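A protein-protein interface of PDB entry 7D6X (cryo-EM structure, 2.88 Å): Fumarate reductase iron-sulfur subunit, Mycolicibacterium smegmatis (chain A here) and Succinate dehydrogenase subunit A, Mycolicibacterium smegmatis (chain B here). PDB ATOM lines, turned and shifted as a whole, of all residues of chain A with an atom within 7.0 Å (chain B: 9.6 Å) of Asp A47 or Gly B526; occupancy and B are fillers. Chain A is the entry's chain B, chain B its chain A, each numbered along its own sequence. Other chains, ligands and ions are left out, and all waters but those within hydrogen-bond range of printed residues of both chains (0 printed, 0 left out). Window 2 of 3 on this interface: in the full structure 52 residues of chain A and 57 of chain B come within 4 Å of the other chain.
The guanidinium group of Arg A99 is in hydrogen-bond range of the backbone carbonyl oxygen of Phe B530. The backbone carbonyl oxygen (O) of Val B529 sits close to the guanidinium group (NH1) of Arg A99. OD2 of Asp A47 sits close to O of Glu B525, 3.4 Å away. The backbone carbonyl oxygen (O) of Pro A46 is in hydrogen-bond range of the side-chain hydroxyl (OH) of Tyr B482 (3.2 Å).
The backbone NH (N) of Ala A49 sits at hydrogen-bond distance from the side-chain carboxylate (OD2) of Asp A100, 3.2 Å away. O of Asp A47 sits at hydrogen-bond distance from NH1 of Arg A99. O of Gly B527 is in hydrogen-bond range of ND2 of Asn B531 (2.9 Å). NH1 of Arg A12 lies within salt-bridge range of OD1 of Asp A47. The guanidinium group of Arg A99 lies within salt-bridge range of the side-chain carboxylate of Asp A100 (3.9 Å). N of Gly B533 lies close to OD1 of Asn B531, at 3.3 Å.
Among the printed residues, pairs that only touch across the chains: Gln A41 with Tyr B482, Gln A41 with Pro B532, Pro A46 with Pro B532, Pro A46 with Gly B533, Asp A47 with Gly B526, Asp A47 with Asn B531, Leu A48 with Pro B532, Ala A49 with Phe B530 and Val A50 with Phe B530.
Of chain B, only Tyr B482, Pro B532 and Gly B533 come within 4 Å of Pro A46. Printed residues of chain B within 4 Å of Leu A48: Pro B532. Printed residues of chain B within 4 Å of Val A50: Phe B530 (3.8 Å). Of the printed residues of chain B, Arg A99 touches Val B529 (3.2 Å) and Phe B530 (2.7 Å). Of the printed residues of chain A, Tyr B482 touches Gln A41 (3.9 Å) and Pro A46 (3.2 Å). Gly B526 touches just one residue of chain A: Asp A47 (3.97 Å). Of the printed residues of chain A, Val B529 touches Arg A99. The nearest residue of chain A that does not touch Gly B526 is Arg A99 (6.0 Å).
Along chain A the printed residues that touch a printed residue of chain B span positions 41 to 99. Of the 20 printed residues of chain B, 8 touch a printed residue of chain A. Hydrophobic or aromatic side chains of chain B within 4 Å of the printed part of chain A: Tyr B482, Phe B530 and Pro B532. Along chain B the printed residues that touch a printed residue of chain A span positions 482 to 533. Among the printed residues, no Asp or Glu carboxylate lies within 4 Å of a Lys or Arg side-chain nitrogen of the other chain.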
ATOM      1  N   ARG A  12      11.704  26.639   8.750  1.00  0.00           N
ATOM      2  CA  ARG A  12      12.713  26.839   7.722  1.00  0.00           C
ATOM      3  C   ARG A  12      12.091  27.599   6.565  1.00  0.00           C
ATOM      4  O   ARG A  12      11.022  27.224   6.081  1.00  0.00           O
ATOM      5  CB  ARG A  12      13.270  25.509   7.215  1.00  0.00           C
ATOM      6  CG  ARG A  12      13.769  24.571   8.279  1.00  0.00           C
ATOM      7  CD  ARG A  12      15.026  25.080   8.926  1.00  0.00           C
ATOM      8  NE  ARG A  12      16.044  25.454   7.954  1.00  0.00           N
ATOM      9  CZ  ARG A  12      16.858  24.597   7.355  1.00  0.00           C
ATOM     10  NH1 ARG A  12      17.758  25.031   6.489  1.00  0.00           N
ATOM     11  NH2 ARG A  12      16.768  23.304   7.619  1.00  0.00           N
ATOM     12  N   GLN A  41      22.956  21.985  13.655  1.00  0.00           N
ATOM     13  CA  GLN A  41      23.820  22.555  12.626  1.00  0.00           C
ATOM     14  C   GLN A  41      25.036  21.679  12.372  1.00  0.00           C
ATOM     15  O   GLN A  41      25.428  21.465  11.222  1.00  0.00           O
ATOM     16  CB  GLN A  41      24.268  23.953  13.035  1.00  0.00           C
ATOM     17  CG  GLN A  41      23.349  25.050  12.588  1.00  0.00           C
ATOM     18  CD  GLN A  41      23.860  26.408  12.984  1.00  0.00           C
ATOM     19  OE1 GLN A  41      24.493  26.564  14.022  1.00  0.00           O
ATOM     20  NE2 GLN A  41      23.593  27.403  12.156  1.00  0.00           N
ATOM     21  N   GLN A  44      23.221  17.873  11.081  1.00  0.00           N
ATOM     22  CA  GLN A  44      22.146  17.664  10.119  1.00  0.00           C
ATOM     23  C   GLN A  44      21.983  18.799   9.121  1.00  0.00           C
ATOM     24  O   GLN A  44      21.990  18.552   7.910  1.00  0.00           O
ATOM     25  CB  GLN A  44      20.818  17.438  10.857  1.00  0.00           C
ATOM     26  CG  GLN A  44      20.674  16.074  11.480  1.00  0.00           C
ATOM     27  CD  GLN A  44      19.325  15.873  12.117  1.00  0.00           C
ATOM     28  OE1 GLN A  44      19.207  15.803  13.336  1.00  0.00           O
ATOM     29  NE2 GLN A  44      18.297  15.774  11.293  1.00  0.00           N
ATOM     30  N   THR A  45      21.822  20.036   9.587  1.00  0.00           N
ATOM     31  CA  THR A  45      21.485  21.168   8.726  1.00  0.00           C
ATOM     32  C   THR A  45      22.532  22.258   8.902  1.00  0.00           C
ATOM     33  O   THR A  45      22.387  23.136   9.761  1.00  0.00           O
ATOM     34  CB  THR A  45      20.092  21.706   9.042  1.00  0.00           C
ATOM     35  OG1 THR A  45      20.108  22.350  10.318  1.00  0.00           O
ATOM     36  CG2 THR A  45      19.096  20.574   9.090  1.00  0.00           C
ATOM     37  N   PRO A  46      23.592  22.247   8.092  1.00  0.00           N
ATOM     38  CA  PRO A  46      24.696  23.191   8.320  1.00  0.00           C
ATOM     39  C   PRO A  46      24.332  24.630   8.036  1.00  0.00           C
ATOM     40  O   PRO A  46      24.949  25.540   8.600  1.00  0.00           O
ATOM     41  CB  PRO A  46      25.782  22.698   7.356  1.00  0.00           C
ATOM     42  CG  PRO A  46      25.324  21.359   6.885  1.00  0.00           C
ATOM     43  CD  PRO A  46      23.847  21.384   6.934  1.00  0.00           C
ATOM     44  N   ASP A  47      23.346  24.866   7.179  1.00  0.00           N
ATOM     45  CA  ASP A  47      22.976  26.206   6.736  1.00  0.00           C
ATOM     46  C   ASP A  47      21.731  26.726   7.435  1.00  0.00           C
ATOM     47  O   ASP A  47      20.920  27.410   6.817  1.00  0.00           O
ATOM     48  CB  ASP A  47      22.771  26.208   5.230  1.00  0.00           C
ATOM     49  CG  ASP A  47      21.961  25.024   4.754  1.00  0.00           C
ATOM     50  OD1 ASP A  47      21.274  24.399   5.585  1.00  0.00           O
ATOM     51  OD2 ASP A  47      22.020  24.697   3.553  1.00  0.00           O
ATOM     52  N   LEU A  48      21.549  26.429   8.716  1.00  0.00           N
ATOM     53  CA  LEU A  48      20.388  26.902   9.456  1.00  0.00           C
ATOM     54  C   LEU A  48      20.731  28.234  10.110  1.00  0.00           C
ATOM     55  O   LEU A  48      21.693  28.327  10.874  1.00  0.00           O
ATOM     56  CB  LEU A  48      19.953  25.869  10.492  1.00  0.00           C
ATOM     57  CG  LEU A  48      18.988  26.269  11.610  1.00  0.00           C
ATOM     58  CD1 LEU A  48      17.557  26.364  11.130  1.00  0.00           C
ATOM     59  CD2 LEU A  48      19.097  25.282  12.752  1.00  0.00           C
ATOM     60  N   ALA A  49      19.955  29.264   9.794  1.00  0.00           N
ATOM     61  CA  ALA A  49      20.207  30.591  10.331  1.00  0.00           C
ATOM     62  C   ALA A  49      19.868  30.645  11.816  1.00  0.00           C
ATOM     63  O   ALA A  49      18.791  30.206  12.222  1.00  0.00           O
ATOM     64  CB  ALA A  49      19.375  31.612   9.564  1.00  0.00           C
ATOM     65  N   VAL A  50      20.778  31.172  12.635  1.00  0.00           N
ATOM     66  CA  VAL A  50      20.508  31.225  14.072  1.00  0.00           C
ATOM     67  C   VAL A  50      20.669  32.626  14.649  1.00  0.00           C
ATOM     68  O   VAL A  50      19.765  33.130  15.324  1.00  0.00           O
ATOM     69  CB  VAL A  50      21.379  30.225  14.850  1.00  0.00           C
ATOM     70  CG1 VAL A  50      21.037  30.299  16.324  1.00  0.00           C
ATOM     71  CG2 VAL A  50      21.133  28.823  14.349  1.00  0.00           C
ATOM     72  N   ARG A  99      15.838  34.840   7.089  1.00  0.00           N
ATOM     73  CA  ARG A  99      15.973  33.431   6.770  1.00  0.00           C
ATOM     74  C   ARG A  99      15.445  32.645   7.965  1.00  0.00           C
ATOM     75  O   ARG A  99      14.702  33.186   8.787  1.00  0.00           O
ATOM     76  CB  ARG A  99      17.419  33.087   6.395  1.00  0.00           C
ATOM     77  CG  ARG A  99      17.486  31.981   5.377  1.00  0.00           C
ATOM     78  CD  ARG A  99      18.849  31.378   5.325  1.00  0.00           C
ATOM     79  NE  ARG A  99      18.846  30.141   4.565  1.00  0.00           N
ATOM     80  CZ  ARG A  99      19.847  29.276   4.572  1.00  0.00           C
ATOM     81  NH1 ARG A  99      20.923  29.522   5.301  1.00  0.00           N
ATOM     82  NH2 ARG A  99      19.773  28.167   3.855  1.00  0.00           N
ATOM     83  N   ASP A 100      15.840  31.375   8.066  1.00  0.00           N
ATOM     84  CA  ASP A 100      15.179  30.392   8.918  1.00  0.00           C
ATOM     85  C   ASP A 100      14.745  30.934  10.276  1.00  0.00           C
ATOM     86  O   ASP A 100      13.549  30.987  10.573  1.00  0.00           O
ATOM     87  CB  ASP A 100      16.109  29.194   9.102  1.00  0.00           C
ATOM     88  CG  ASP A 100      16.591  28.630   7.787  1.00  0.00           C
ATOM     89  OD1 ASP A 100      15.832  28.662   6.802  1.00  0.00           O
ATOM     90  OD2 ASP A 100      17.733  28.147   7.735  1.00  0.00           O
ATOM     91  N   LEU B 469      34.787  32.781  -2.290  1.00  0.00           N
ATOM     92  CA  LEU B 469      33.836  31.900  -2.958  1.00  0.00           C
ATOM     93  C   LEU B 469      34.391  30.512  -3.242  1.00  0.00           C
ATOM     94  O   LEU B 469      33.682  29.687  -3.821  1.00  0.00           O
ATOM     95  CB  LEU B 469      33.369  32.530  -4.269  1.00  0.00           C
ATOM     96  CG  LEU B 469      32.433  33.723  -4.160  1.00  0.00           C
ATOM     97  CD1 LEU B 469      32.000  34.153  -5.540  1.00  0.00           C
ATOM     98  CD2 LEU B 469      31.238  33.383  -3.300  1.00  0.00           C
ATOM     99  N   PRO B 471      34.937  27.932  -1.177  1.00  0.00           N
ATOM    100  CA  PRO B 471      34.262  26.795  -0.537  1.00  0.00           C
ATOM    101  C   PRO B 471      32.958  26.368  -1.189  1.00  0.00           C
ATOM    102  O   PRO B 471      32.256  25.514  -0.647  1.00  0.00           O
ATOM    103  CB  PRO B 471      34.015  27.300   0.889  1.00  0.00           C
ATOM    104  CG  PRO B 471      34.118  28.756   0.809  1.00  0.00           C
ATOM    105  CD  PRO B 471      35.171  29.004  -0.199  1.00  0.00           C
ATOM    106  N   PHE B 472      32.616  26.942  -2.333  1.00  0.00           N
ATOM    107  CA  PHE B 472      31.399  26.600  -3.059  1.00  0.00           C
ATOM    108  C   PHE B 472      31.721  25.820  -4.327  1.00  0.00           C
ATOM    109  O   PHE B 472      31.110  26.030  -5.375  1.00  0.00           O
ATOM    110  CB  PHE B 472      30.599  27.852  -3.396  1.00  0.00           C
ATOM    111  CG  PHE B 472      29.803  28.390  -2.250  1.00  0.00           C
ATOM    112  CD1 PHE B 472      30.077  29.632  -1.727  1.00  0.00           C
ATOM    113  CD2 PHE B 472      28.775  27.656  -1.701  1.00  0.00           C
ATOM    114  CE1 PHE B 472      29.349  30.123  -0.678  1.00  0.00           C
ATOM    115  CE2 PHE B 472      28.046  28.149  -0.652  1.00  0.00           C
ATOM    116  CZ  PHE B 472      28.332  29.382  -0.142  1.00  0.00           C
ATOM    117  N   GLU B 473      32.691  24.923  -4.250  1.00  0.00           N
ATOM    118  CA  GLU B 473      33.085  24.072  -5.359  1.00  0.00           C
ATOM    119  C   GLU B 473      32.899  22.604  -4.990  1.00  0.00           C
ATOM    120  O   GLU B 473      32.748  22.268  -3.810  1.00  0.00           O
ATOM    121  CB  GLU B 473      34.545  24.334  -5.746  1.00  0.00           C
ATOM    122  CG  GLU B 473      34.713  25.432  -6.769  1.00  0.00           C
ATOM    123  CD  GLU B 473      36.147  25.899  -6.889  1.00  0.00           C
ATOM    124  OE1 GLU B 473      37.055  25.041  -6.872  1.00  0.00           O
ATOM    125  OE2 GLU B 473      36.366  27.123  -6.996  1.00  0.00           O
ATOM    126  N   ASN B 480      34.264  19.181   6.041  1.00  0.00           N
ATOM    127  CA  ASN B 480      33.138  19.889   6.617  1.00  0.00           C
ATOM    128  C   ASN B 480      33.663  20.979   7.540  1.00  0.00           C
ATOM    129  O   ASN B 480      34.622  20.748   8.280  1.00  0.00           O
ATOM    130  CB  ASN B 480      32.231  18.930   7.398  1.00  0.00           C
ATOM    131  CG  ASN B 480      30.862  19.503   7.659  1.00  0.00           C
ATOM    132  OD1 ASN B 480      30.213  20.015   6.754  1.00  0.00           O
ATOM    133  ND2 ASN B 480      30.406  19.412   8.899  1.00  0.00           N
ATOM    134  N   PRO B 481      33.076  22.175   7.506  1.00  0.00           N
ATOM    135  CA  PRO B 481      33.572  23.246   8.383  1.00  0.00           C
ATOM    136  C   PRO B 481      33.531  22.886   9.854  1.00  0.00           C
ATOM    137  O   PRO B 481      34.463  23.209  10.600  1.00  0.00           O
ATOM    138  CB  PRO B 481      32.631  24.413   8.065  1.00  0.00           C
ATOM    139  CG  PRO B 481      32.094  24.120   6.726  1.00  0.00           C
ATOM    140  CD  PRO B 481      32.001  22.641   6.618  1.00  0.00           C
ATOM    141  N   TYR B 482      32.473  22.205  10.289  1.00  0.00           N
ATOM    142  CA  TYR B 482      32.289  21.947  11.710  1.00  0.00           C
ATOM    143  C   TYR B 482      33.219  20.848  12.201  1.00  0.00           C
ATOM    144  O   TYR B 482      33.728  20.915  13.324  1.00  0.00           O
ATOM    145  CB  TYR B 482      30.834  21.591  11.976  1.00  0.00           C
ATOM    146  CG  TYR B 482      29.885  22.703  11.630  1.00  0.00           C
ATOM    147  CD1 TYR B 482      29.615  23.709  12.536  1.00  0.00           C
ATOM    148  CD2 TYR B 482      29.266  22.755  10.396  1.00  0.00           C
ATOM    149  CE1 TYR B 482      28.755  24.729  12.228  1.00  0.00           C
ATOM    150  CE2 TYR B 482      28.403  23.774  10.081  1.00  0.00           C
ATOM    151  CZ  TYR B 482      28.155  24.757  11.003  1.00  0.00           C
ATOM    152  OH  TYR B 482      27.295  25.777  10.705  1.00  0.00           O
ATOM    153  N   THR B 523      34.056  22.167   1.918  1.00  0.00           N
ATOM    154  CA  THR B 523      32.917  22.420   1.052  1.00  0.00           C
ATOM    155  C   THR B 523      31.742  22.893   1.883  1.00  0.00           C
ATOM    156  O   THR B 523      31.471  22.350   2.956  1.00  0.00           O
ATOM    157  CB  THR B 523      32.499  21.186   0.280  1.00  0.00           C
ATOM    158  OG1 THR B 523      32.003  20.204   1.196  1.00  0.00           O
ATOM    159  CG2 THR B 523      33.668  20.617  -0.452  1.00  0.00           C
ATOM    160  N   VAL B 524      31.047  23.901   1.374  1.00  0.00           N
ATOM    161  CA  VAL B 524      29.862  24.455   2.008  1.00  0.00           C
ATOM    162  C   VAL B 524      28.659  24.036   1.183  1.00  0.00           C
ATOM    163  O   VAL B 524      28.701  24.079  -0.051  1.00  0.00           O
ATOM    164  CB  VAL B 524      29.954  25.983   2.124  1.00  0.00           C
ATOM    165  CG1 VAL B 524      28.731  26.531   2.797  1.00  0.00           C
ATOM    166  CG2 VAL B 524      31.184  26.365   2.897  1.00  0.00           C
ATOM    167  N   GLU B 525      27.600  23.615   1.861  1.00  0.00           N
ATOM    168  CA  GLU B 525      26.357  23.226   1.215  1.00  0.00           C
ATOM    169  C   GLU B 525      25.368  24.380   1.290  1.00  0.00           C
ATOM    170  O   GLU B 525      25.189  24.979   2.353  1.00  0.00           O
ATOM    171  CB  GLU B 525      25.772  21.981   1.880  1.00  0.00           C
ATOM    172  CG  GLU B 525      26.726  20.804   1.941  1.00  0.00           C
ATOM    173  CD  GLU B 525      27.153  20.324   0.566  1.00  0.00           C
ATOM    174  OE1 GLU B 525      26.353  20.441  -0.386  1.00  0.00           O
ATOM    175  OE2 GLU B 525      28.292  19.828   0.434  1.00  0.00           O
ATOM    176  N   GLY B 526      24.740  24.690   0.172  1.00  0.00           N
ATOM    177  CA  GLY B 526      23.734  25.722   0.126  1.00  0.00           C
ATOM    178  C   GLY B 526      24.164  26.930  -0.681  1.00  0.00           C
ATOM    179  O   GLY B 526      25.088  26.883  -1.495  1.00  0.00           O
ATOM    180  N   GLY B 527      23.460  28.036  -0.447  1.00  0.00           N
ATOM    181  CA  GLY B 527      23.747  29.290  -1.102  1.00  0.00           C
ATOM    182  C   GLY B 527      24.465  30.262  -0.184  1.00  0.00           C
ATOM    183  O   GLY B 527      25.031  29.898   0.847  1.00  0.00           O
ATOM    184  N   ARG B 528      24.428  31.528  -0.576  1.00  0.00           N
ATOM    185  CA  ARG B 528      25.131  32.573   0.147  1.00  0.00           C
ATOM    186  C   ARG B 528      24.234  33.359   1.088  1.00  0.00           C
ATOM    187  O   ARG B 528      24.736  34.194   1.842  1.00  0.00           O
ATOM    188  CB  ARG B 528      25.801  33.522  -0.840  1.00  0.00           C
ATOM    189  CG  ARG B 528      26.942  32.882  -1.588  1.00  0.00           C
ATOM    190  CD  ARG B 528      27.237  33.615  -2.870  1.00  0.00           C
ATOM    191  NE  ARG B 528      27.524  35.020  -2.627  1.00  0.00           N
ATOM    192  CZ  ARG B 528      27.903  35.872  -3.569  1.00  0.00           C
ATOM    193  NH1 ARG B 528      28.144  37.133  -3.258  1.00  0.00           N
ATOM    194  NH2 ARG B 528      28.038  35.463  -4.821  1.00  0.00           N
ATOM    195  N   VAL B 529      22.929  33.103   1.087  1.00  0.00           N
ATOM    196  CA  VAL B 529      22.005  33.879   1.906  1.00  0.00           C
ATOM    197  C   VAL B 529      22.088  33.349   3.334  1.00  0.00           C
ATOM    198  O   VAL B 529      21.417  32.381   3.690  1.00  0.00           O
ATOM    199  CB  VAL B 529      20.579  33.823   1.361  1.00  0.00           C
ATOM    200  CG1 VAL B 529      19.680  34.738   2.147  1.00  0.00           C
ATOM    201  CG2 VAL B 529      20.570  34.200  -0.107  1.00  0.00           C
ATOM    202  N   PHE B 530      22.908  34.001   4.153  1.00  0.00           N
ATOM    203  CA  PHE B 530      23.112  33.693   5.568  1.00  0.00           C
ATOM    204  C   PHE B 530      23.369  32.198   5.777  1.00  0.00           C
ATOM    205  O   PHE B 530      22.563  31.467   6.343  1.00  0.00           O
ATOM    206  CB  PHE B 530      21.929  34.151   6.415  1.00  0.00           C
ATOM    207  CG  PHE B 530      22.250  34.262   7.870  1.00  0.00           C
ATOM    208  CD1 PHE B 530      22.693  35.452   8.399  1.00  0.00           C
ATOM    209  CD2 PHE B 530      22.194  33.165   8.691  1.00  0.00           C
ATOM    210  CE1 PHE B 530      23.000  35.560   9.736  1.00  0.00           C
ATOM    211  CE2 PHE B 530      22.509  33.265  10.029  1.00  0.00           C
ATOM    212  CZ  PHE B 530      22.918  34.456  10.547  1.00  0.00           C
ATOM    213  N   ASN B 531      24.517  31.762   5.273  1.00  0.00           N
ATOM    214  CA  ASN B 531      24.938  30.372   5.381  1.00  0.00           C
ATOM    215  C   ASN B 531      26.028  30.278   6.433  1.00  0.00           C
ATOM    216  O   ASN B 531      27.204  30.506   6.122  1.00  0.00           O
ATOM    217  CB  ASN B 531      25.446  29.869   4.029  1.00  0.00           C
ATOM    218  CG  ASN B 531      25.602  28.375   3.980  1.00  0.00           C
ATOM    219  OD1 ASN B 531      25.666  27.710   5.005  1.00  0.00           O
ATOM    220  ND2 ASN B 531      25.669  27.834   2.777  1.00  0.00           N
ATOM    221  N   PRO B 532      25.700  29.966   7.689  1.00  0.00           N
ATOM    222  CA  PRO B 532      26.741  29.926   8.727  1.00  0.00           C
ATOM    223  C   PRO B 532      27.817  28.884   8.487  1.00  0.00           C
ATOM    224  O   PRO B 532      28.920  29.022   9.027  1.00  0.00           O
ATOM    225  CB  PRO B 532      25.946  29.642  10.007  1.00  0.00           C
ATOM    226  CG  PRO B 532      24.625  29.177   9.562  1.00  0.00           C
ATOM    227  CD  PRO B 532      24.358  29.830   8.262  1.00  0.00           C
ATOM    228  N   GLY B 533      27.545  27.848   7.696  1.00  0.00           N
ATOM    229  CA  GLY B 533      28.618  26.966   7.278  1.00  0.00           C
ATOM    230  C   GLY B 533      29.646  27.686   6.430  1.00  0.00           C
ATOM    231  O   GLY B 533      30.850  27.468   6.573  1.00  0.00           O
ATOM    232  N   TRP B 534      29.182  28.571   5.548  1.00  0.00           N
ATOM    233  CA  TRP B 534      30.082  29.397   4.756  1.00  0.00           C
ATOM    234  C   TRP B 534      30.882  30.340   5.643  1.00  0.00           C
ATOM    235  O   TRP B 534      32.094  30.500   5.463  1.00  0.00           O
ATOM    236  CB  TRP B 534      29.264  30.174   3.729  1.00  0.00           C
ATOM    237  CG  TRP B 534      30.039  31.024   2.790  1.00  0.00           C
ATOM    238  CD1 TRP B 534      31.208  30.716   2.174  1.00  0.00           C
ATOM    239  CD2 TRP B 534      29.680  32.329   2.338  1.00  0.00           C
ATOM    240  NE1 TRP B 534      31.607  31.750   1.373  1.00  0.00           N
ATOM    241  CE2 TRP B 534      30.683  32.756   1.460  1.00  0.00           C
ATOM    242  CE3 TRP B 534      28.607  33.183   2.600  1.00  0.00           C
ATOM    243  CZ2 TRP B 534      30.647  33.996   0.839  1.00  0.00           C
ATOM    244  CZ3 TRP B 534      28.575  34.407   1.986  1.00  0.00           C
ATOM    245  CH2 TRP B 534      29.585  34.804   1.115  1.00  0.00           C
ATOM    246  N   HIS B 535      30.222  30.964   6.616  1.00  0.00           N
ATOM    247  CA  HIS B 535      30.916  31.865   7.524  1.00  0.00           C
ATOM    248  C   HIS B 535      31.994  31.133   8.309  1.00  0.00           C
ATOM    249  O   HIS B 535      33.098  31.657   8.509  1.00  0.00           O
ATOM    250  CB  HIS B 535      29.913  32.522   8.468  1.00  0.00           C
ATOM    251  CG  HIS B 535      28.771  33.197   7.769  1.00  0.00           C
ATOM    252  ND1 HIS B 535      27.664  33.665   8.442  1.00  0.00           N
ATOM    253  CD2 HIS B 535      28.567  33.487   6.465  1.00  0.00           C
ATOM    254  CE1 HIS B 535      26.827  34.210   7.581  1.00  0.00           C
ATOM    255  NE2 HIS B 535      27.350  34.115   6.375  1.00  0.00           N
